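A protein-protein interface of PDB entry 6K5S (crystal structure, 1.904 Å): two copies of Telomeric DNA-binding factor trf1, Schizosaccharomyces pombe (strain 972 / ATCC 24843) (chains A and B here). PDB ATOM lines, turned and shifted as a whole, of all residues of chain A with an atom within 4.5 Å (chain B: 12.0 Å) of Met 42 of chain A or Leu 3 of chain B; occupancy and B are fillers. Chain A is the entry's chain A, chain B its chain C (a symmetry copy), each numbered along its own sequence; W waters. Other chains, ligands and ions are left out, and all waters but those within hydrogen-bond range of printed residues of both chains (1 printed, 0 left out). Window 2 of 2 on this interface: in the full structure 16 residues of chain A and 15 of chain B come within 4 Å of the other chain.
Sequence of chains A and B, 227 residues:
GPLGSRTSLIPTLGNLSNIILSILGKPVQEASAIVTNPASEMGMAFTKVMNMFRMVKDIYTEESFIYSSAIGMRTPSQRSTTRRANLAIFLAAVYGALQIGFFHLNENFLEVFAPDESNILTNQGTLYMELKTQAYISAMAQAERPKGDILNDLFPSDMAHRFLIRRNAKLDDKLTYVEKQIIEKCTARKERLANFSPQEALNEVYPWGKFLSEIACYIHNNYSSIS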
ATOM      1  N   SER A  22      31.891   5.150  18.080  1.00  0.00           N
ATOM      2  CA  SER A  22      31.280   6.251  17.354  1.00  0.00           C
ATOM      3  C   SER A  22      31.513   7.589  18.041  1.00  0.00           C
ATOM      4  O   SER A  22      31.524   8.627  17.369  1.00  0.00           O
ATOM      5  CB  SER A  22      29.790   5.981  17.161  1.00  0.00           C
ATOM      6  OG  SER A  22      29.091   6.133  18.374  1.00  0.00           O
ATOM      7  N   ILE A  23      31.727   7.602  19.360  1.00  0.00           N
ATOM      8  CA  ILE A  23      32.126   8.849  20.004  1.00  0.00           C
ATOM      9  C   ILE A  23      33.578   9.171  19.676  1.00  0.00           C
ATOM     10  O   ILE A  23      33.890  10.261  19.175  1.00  0.00           O
ATOM     11  CB  ILE A  23      31.880   8.798  21.522  1.00  0.00           C
ATOM     12  CG1 ILE A  23      30.389   8.823  21.829  1.00  0.00           C
ATOM     13  CG2 ILE A  23      32.548  10.006  22.210  1.00  0.00           C
ATOM     14  CD1 ILE A  23      30.077   8.726  23.326  1.00  0.00           C
ATOM     15  N   ILE A  34      35.620  15.802  24.004  1.00  0.00           N
ATOM     16  CA  ILE A  34      34.726  15.016  24.841  1.00  0.00           C
ATOM     17  C   ILE A  34      35.496  14.420  26.016  1.00  0.00           C
ATOM     18  O   ILE A  34      35.074  14.530  27.177  1.00  0.00           O
ATOM     19  CB  ILE A  34      34.025  13.958  23.966  1.00  0.00           C
ATOM     20  CG1 ILE A  34      33.143  14.678  22.937  1.00  0.00           C
ATOM     21  CG2 ILE A  34      33.227  12.990  24.803  1.00  0.00           C
ATOM     22  CD1 ILE A  34      32.439  13.788  21.941  1.00  0.00           C
ATOM     23  N   SER A  40      31.143  18.625  30.328  1.00  0.00           N
ATOM     24  CA  SER A  40      30.250  19.001  29.241  1.00  0.00           C
ATOM     25  C   SER A  40      29.122  17.979  29.126  1.00  0.00           C
ATOM     26  O   SER A  40      29.145  16.921  29.759  1.00  0.00           O
ATOM     27  CB  SER A  40      31.028  19.116  27.932  1.00  0.00           C
ATOM     28  OG  SER A  40      31.522  17.854  27.522  1.00  0.00           O
ATOM     29  N   GLU A  41      28.105  18.308  28.327  1.00  0.00           N
ATOM     30  CA  GLU A  41      26.976  17.391  28.186  1.00  0.00           C
ATOM     31  C   GLU A  41      27.440  16.051  27.622  1.00  0.00           C
ATOM     32  O   GLU A  41      27.231  14.999  28.239  1.00  0.00           O
ATOM     33  CB  GLU A  41      25.894  18.013  27.303  1.00  0.00           C
ATOM     34  CG  GLU A  41      24.706  17.082  27.026  1.00  0.00           C
ATOM     35  CD  GLU A  41      23.582  17.779  26.255  1.00  0.00           C
ATOM     36  OE1 GLU A  41      23.542  19.025  26.283  1.00  0.00           O
ATOM     37  OE2 GLU A  41      22.751  17.079  25.629  1.00  0.00           O
ATOM     38  N   MET A  42      28.116  16.084  26.473  1.00  0.00           N
ATOM     39  CA  MET A  42      28.623  14.864  25.869  1.00  0.00           C
ATOM     40  C   MET A  42      29.735  14.235  26.703  1.00  0.00           C
ATOM     41  O   MET A  42      29.853  13.008  26.725  1.00  0.00           O
ATOM     42  CB  MET A  42      29.109  15.137  24.446  1.00  0.00           C
ATOM     43  CG  MET A  42      27.974  15.154  23.387  1.00  0.00           C
ATOM     44  SD  MET A  42      27.140  13.545  23.138  1.00  0.00           S
ATOM     45  CE  MET A  42      28.459  12.385  23.467  1.00  0.00           C
ATOM     46  N   GLY A  43      30.549  15.052  27.387  1.00  0.00           N
ATOM     47  CA  GLY A  43      31.620  14.508  28.213  1.00  0.00           C
ATOM     48  C   GLY A  43      31.091  13.691  29.372  1.00  0.00           C
ATOM     49  O   GLY A  43      31.636  12.629  29.700  1.00  0.00           O
ATOM     50  N   MET A  44      30.024  14.183  30.015  1.00  0.00           N
ATOM     51  CA  MET A  44      29.381  13.466  31.108  1.00  0.00           C
ATOM     52  C   MET A  44      28.772  12.159  30.624  1.00  0.00           C
ATOM     53  O   MET A  44      28.802  11.150  31.337  1.00  0.00           O
ATOM     54  CB  MET A  44      28.277  14.328  31.741  1.00  0.00           C
ATOM     55  CG  MET A  44      28.737  15.553  32.534  1.00  0.00           C
ATOM     56  SD  MET A  44      27.266  16.490  33.074  1.00  0.00           S
ATOM     57  CE  MET A  44      26.303  15.136  33.733  1.00  0.00           C
ATOM     58  N   ALA A  45      28.166  12.174  29.433  1.00  0.00           N
ATOM     59  CA  ALA A  45      27.580  10.956  28.883  1.00  0.00           C
ATOM     60  C   ALA A  45      28.668   9.948  28.535  1.00  0.00           C
ATOM     61  O   ALA A  45      28.501   8.741  28.758  1.00  0.00           O
ATOM     62  CB  ALA A  45      26.738  11.290  27.654  1.00  0.00           C
ATOM     63  N   PHE A  46      29.796  10.427  28.004  1.00  0.00           N
ATOM     64  CA  PHE A  46      30.923   9.539  27.729  1.00  0.00           C
ATOM     65  C   PHE A  46      31.473   8.932  29.014  1.00  0.00           C
ATOM     66  O   PHE A  46      31.804   7.740  29.045  1.00  0.00           O
ATOM     67  CB  PHE A  46      32.019  10.299  26.976  1.00  0.00           C
ATOM     68  CG  PHE A  46      33.247   9.481  26.683  1.00  0.00           C
ATOM     69  CD1 PHE A  46      33.240   8.532  25.682  1.00  0.00           C
ATOM     70  CD2 PHE A  46      34.414   9.658  27.424  1.00  0.00           C
ATOM     71  CE1 PHE A  46      34.379   7.775  25.402  1.00  0.00           C
ATOM     72  CE2 PHE A  46      35.564   8.895  27.145  1.00  0.00           C
ATOM     73  CZ  PHE A  46      35.534   7.955  26.133  1.00  0.00           C
ATOM     74  N   GLY B   1      17.867  10.140  20.183  1.00  0.00           N
ATOM     75  CA  GLY B   1      18.646  11.110  20.930  1.00  0.00           C
ATOM     76  C   GLY B   1      20.106  11.140  20.519  1.00  0.00           C
ATOM     77  O   GLY B   1      20.516  10.414  19.605  1.00  0.00           O
ATOM     78  N   PRO B   2      20.892  11.986  21.180  1.00  0.00           N
ATOM     79  CA  PRO B   2      22.327  12.044  20.885  1.00  0.00           C
ATOM     80  C   PRO B   2      23.041  10.736  21.202  1.00  0.00           C
ATOM     81  O   PRO B   2      22.570   9.899  21.975  1.00  0.00           O
ATOM     82  CB  PRO B   2      22.832  13.181  21.781  1.00  0.00           C
ATOM     83  CG  PRO B   2      21.709  13.447  22.766  1.00  0.00           C
ATOM     84  CD  PRO B   2      20.459  13.095  22.045  1.00  0.00           C
ATOM     85  N   LEU B   3      24.198  10.577  20.565  1.00  0.00           N
ATOM     86  CA  LEU B   3      25.096   9.466  20.833  1.00  0.00           C
ATOM     87  C   LEU B   3      25.371   9.305  22.325  1.00  0.00           C
ATOM     88  O   LEU B   3      25.756  10.261  23.007  1.00  0.00           O
ATOM     89  CB  LEU B   3      26.395   9.733  20.089  1.00  0.00           C
ATOM     90  CG  LEU B   3      27.296   8.583  19.720  1.00  0.00           C
ATOM     91  CD1 LEU B   3      26.443   7.361  19.347  1.00  0.00           C
ATOM     92  CD2 LEU B   3      28.145   9.079  18.571  1.00  0.00           C
ATOM     93  N   GLY B   4      25.198   8.083  22.831  1.00  0.00           N
ATOM     94  CA  GLY B   4      25.479   7.804  24.227  1.00  0.00           C
ATOM     95  C   GLY B   4      24.409   8.252  25.196  1.00  0.00           C
ATOM     96  O   GLY B   4      24.632   8.212  26.413  1.00  0.00           O
ATOM     97  N   SER B   5      23.262   8.678  24.710  1.00  0.00           N
ATOM     98  CA  SER B   5      22.172   9.071  25.576  1.00  0.00           C
ATOM     99  C   SER B   5      21.221   7.888  25.775  1.00  0.00           C
ATOM    100  O   SER B   5      21.577   6.732  25.512  1.00  0.00           O
ATOM    101  CB  SER B   5      21.475  10.287  24.983  1.00  0.00           C
ATOM    102  OG  SER B   5      21.003   9.990  23.677  1.00  0.00           O
ATOM    103  N   ARG B   6      20.012   8.179  26.257  1.00  0.00           N
ATOM    104  CA  ARG B   6      19.050   7.141  26.624  1.00  0.00           C
ATOM    105  C   ARG B   6      18.656   6.265  25.444  1.00  0.00           C
ATOM    106  O   ARG B   6      18.499   5.047  25.606  1.00  0.00           O
ATOM    107  CB  ARG B   6      17.804   7.779  27.249  1.00  0.00           C
ATOM    108  CG  ARG B   6      18.074   8.337  28.657  1.00  0.00           C
ATOM    109  CD  ARG B   6      16.934   9.223  29.163  1.00  0.00           C
ATOM    110  NE  ARG B   6      17.136   9.549  30.573  1.00  0.00           N
ATOM    111  CZ  ARG B   6      16.688  10.653  31.161  1.00  0.00           C
ATOM    112  NH1 ARG B   6      15.998  11.555  30.461  1.00  0.00           N
ATOM    113  NH2 ARG B   6      16.937  10.858  32.445  1.00  0.00           N
ATOM    114  N   THR B   7      18.481   6.843  24.244  1.00  0.00           N
ATOM    115  CA  THR B   7      18.127   5.963  23.133  1.00  0.00           C
ATOM    116  C   THR B   7      19.315   5.103  22.717  1.00  0.00           C
ATOM    117  O   THR B   7      19.108   3.981  22.252  1.00  0.00           O
ATOM    118  CB  THR B   7      17.607   6.725  21.892  1.00  0.00           C
ATOM    119  OG1 THR B   7      18.648   7.524  21.356  1.00  0.00           O
ATOM    120  CG2 THR B   7      16.393   7.602  22.219  1.00  0.00           C
ATOM    121  N   SER B   8      20.555   5.612  22.857  1.00  0.00           N
ATOM    122  CA  SER B   8      21.720   4.817  22.456  1.00  0.00           C
ATOM    123  C   SER B   8      21.908   3.586  23.340  1.00  0.00           C
ATOM    124  O   SER B   8      22.437   2.569  22.879  1.00  0.00           O
ATOM    125  CB  SER B   8      23.019   5.648  22.502  1.00  0.00           C
ATOM    126  OG  SER B   8      22.959   6.778  21.664  1.00  0.00           O
ATOM    127  N   LEU B   9      21.537   3.670  24.615  1.00  0.00           N
ATOM    128  CA  LEU B   9      21.835   2.624  25.579  1.00  0.00           C
ATOM    129  C   LEU B   9      20.700   1.616  25.733  1.00  0.00           C
ATOM    130  O   LEU B   9      20.807   0.716  26.575  1.00  0.00           O
ATOM    131  CB  LEU B   9      22.176   3.235  26.942  1.00  0.00           C
ATOM    132  CG  LEU B   9      23.574   3.863  27.043  1.00  0.00           C
ATOM    133  CD1 LEU B   9      23.711   4.769  28.261  1.00  0.00           C
ATOM    134  CD2 LEU B   9      24.683   2.789  27.065  1.00  0.00           C
ATOM    135  N   ILE B  10      19.642   1.719  24.928  1.00  0.00           N
ATOM    136  CA  ILE B  10      18.485   0.819  25.011  1.00  0.00           C
ATOM    137  C   ILE B  10      18.894  -0.650  24.948  1.00  0.00           C
ATOM    138  O   ILE B  10      18.376  -1.442  25.741  1.00  0.00           O
ATOM    139  CB  ILE B  10      17.438   1.140  23.930  1.00  0.00           C
ATOM    140  CG1 ILE B  10      16.669   2.386  24.352  1.00  0.00           C
ATOM    141  CG2 ILE B  10      16.447  -0.048  23.770  1.00  0.00           C
ATOM    142  CD1 ILE B  10      15.762   2.144  25.544  1.00  0.00           C
ATOM    143  N   PRO B  11      19.798  -1.077  24.057  1.00  0.00           N
ATOM    144  CA  PRO B  11      20.197  -2.495  24.086  1.00  0.00           C
ATOM    145  C   PRO B  11      20.844  -2.914  25.396  1.00  0.00           C
ATOM    146  O   PRO B  11      20.654  -4.053  25.825  1.00  0.00           O
ATOM    147  CB  PRO B  11      21.177  -2.618  22.907  1.00  0.00           C
ATOM    148  CG  PRO B  11      20.857  -1.464  22.019  1.00  0.00           C
ATOM    149  CD  PRO B  11      20.459  -0.357  22.945  1.00  0.00           C
ATOM    150  N   THR B  12      21.613  -2.045  26.048  1.00  0.00           N
ATOM    151  CA  THR B  12      22.225  -2.432  27.320  1.00  0.00           C
ATOM    152  C   THR B  12      21.159  -2.569  28.397  1.00  0.00           C
ATOM    153  O   THR B  12      21.167  -3.527  29.183  1.00  0.00           O
ATOM    154  CB  THR B  12      23.294  -1.399  27.748  1.00  0.00           C
ATOM    155  OG1 THR B  12      24.446  -1.490  26.906  1.00  0.00           O
ATOM    156  CG2 THR B  12      23.752  -1.648  29.187  1.00  0.00           C
ATOM    157  N   ILE B  59      20.709   6.185  34.547  1.00  0.00           N
ATOM    158  CA  ILE B  59      20.687   6.961  33.321  1.00  0.00           C
ATOM    159  C   ILE B  59      19.254   7.196  32.871  1.00  0.00           C
ATOM    160  O   ILE B  59      18.942   8.231  32.272  1.00  0.00           O
ATOM    161  CB  ILE B  59      21.541   6.253  32.248  1.00  0.00           C
ATOM    162  CG1 ILE B  59      23.004   6.223  32.699  1.00  0.00           C
ATOM    163  CG2 ILE B  59      21.404   6.945  30.878  1.00  0.00           C
ATOM    164  CD1 ILE B  59      23.893   5.388  31.821  1.00  0.00           C
ATOM    165  N   TYR B  60      18.353   6.263  33.170  1.00  0.00           N
ATOM    166  CA  TYR B  60      16.977   6.340  32.703  1.00  0.00           C
ATOM    167  C   TYR B  60      16.012   6.948  33.715  1.00  0.00           C
ATOM    168  O   TYR B  60      14.917   7.364  33.318  1.00  0.00           O
ATOM    169  CB  TYR B  60      16.465   4.941  32.294  1.00  0.00           C
ATOM    170  CG  TYR B  60      17.072   4.475  30.988  1.00  0.00           C
ATOM    171  CD1 TYR B  60      16.469   4.777  29.769  1.00  0.00           C
ATOM    172  CD2 TYR B  60      18.270   3.780  30.970  1.00  0.00           C
ATOM    173  CE1 TYR B  60      17.042   4.375  28.576  1.00  0.00           C
ATOM    174  CE2 TYR B  60      18.845   3.371  29.795  1.00  0.00           C
ATOM    175  CZ  TYR B  60      18.232   3.686  28.592  1.00  0.00           C
ATOM    176  OH  TYR B  60      18.800   3.269  27.423  1.00  0.00           O
ATOM    177  N   MET B  73      11.133   8.240  25.562  1.00  0.00           N
ATOM    178  CA  MET B  73      11.403   7.002  24.830  1.00  0.00           C
ATOM    179  C   MET B  73      10.178   6.713  23.968  1.00  0.00           C
ATOM    180  O   MET B  73       9.207   6.087  24.404  1.00  0.00           O
ATOM    181  CB  MET B  73      11.732   5.864  25.792  1.00  0.00           C
ATOM    182  CG  MET B  73      13.082   6.032  26.537  1.00  0.00           C
ATOM    183  SD  MET B  73      14.579   6.050  25.512  1.00  0.00           S
ATOM    184  CE  MET B  73      14.775   7.822  25.323  1.00  0.00           C
ATOM    185  N   GLN B  78      11.712   0.979  22.182  1.00  0.00           N
ATOM    186  CA  GLN B  78      12.130   1.711  23.372  1.00  0.00           C
ATOM    187  C   GLN B  78      11.103   1.570  24.492  1.00  0.00           C
ATOM    188  O   GLN B  78      11.460   1.362  25.658  1.00  0.00           O
ATOM    189  CB  GLN B  78      12.357   3.188  23.021  1.00  0.00           C
ATOM    190  CG  GLN B  78      13.651   3.431  22.257  1.00  0.00           C
ATOM    191  CD  GLN B  78      13.710   4.750  21.493  1.00  0.00           C
ATOM    192  OE1 GLN B  78      12.870   5.642  21.661  1.00  0.00           O
ATOM    193  NE2 GLN B  78      14.735   4.884  20.651  1.00  0.00           N
HETATM  194  O   HOH W   1      25.618   8.107  28.912  1.00  0.00           O
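The side-chain sulfur of Met 42 of chain A lies close to the backbone carbonyl oxygen of Leu 3 of chain B, at 3.6 Å.
The side-chain hydroxyl (OG) of Ser 8 of chain B sits at hydrogen-bond distance from the backbone NH (N) of Gly 4 of chain B, 2.8 Å away.
Leu 3 of chain B touches Ser 22 of chain A. Ile 23 of chain A touches Leu 3 of chain B. Ala 45 of chain A touches Gly 4 of chain B.
Ser 22 of chain A touches just one residue of chain B: Leu 3. Glu 41 of chain A touches none of the printed residues of chain B. Met 42 of chain A touches one residue of chain B. No residue of chain B comes within 4 Å of Gly 43 of chain A. No residue of chain B comes within 4 Å of Met 44 of chain A. Ala 45 of chain A touches just one residue of chain B: Gly 4 (3.9 Å). Phe 46 of chain A touches none of the printed residues of chain B. Leu 3 of chain B touches just these residues of chain A: Ser 22 (3.1 Å), Ile 23 (3.8 Å) and Met 42 (3.5 Å). Of the printed residues of chain A, Gly 4 of chain B touches Ala 45.
Hydrophobic or aromatic side chains of chain B within 4 Å of the printed part of chain A: Leu 3. Along chain B the printed residues that touch a printed residue of chain A span positions 3 to 4. Hydrophobic or aromatic side chains of chain A within 4 Å of the printed part of chain B: Ile 23, Met 42 and Ala 45. Among the printed residues, no Asp or Glu carboxylate lies within 4 Å of a Lys or Arg side-chain nitrogen of the other chain.
No position is printed for both chains. Of the 4 pairs that touch across the chains among the printed residues, none has its exchanged pair printed and touching as well.
Water W1 bridges the backbone carbonyl oxygen of Gly 4 of chain B (2.7 Å) and the backbone carbonyl oxygen of Ala 45 of chain A (3.0 Å).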
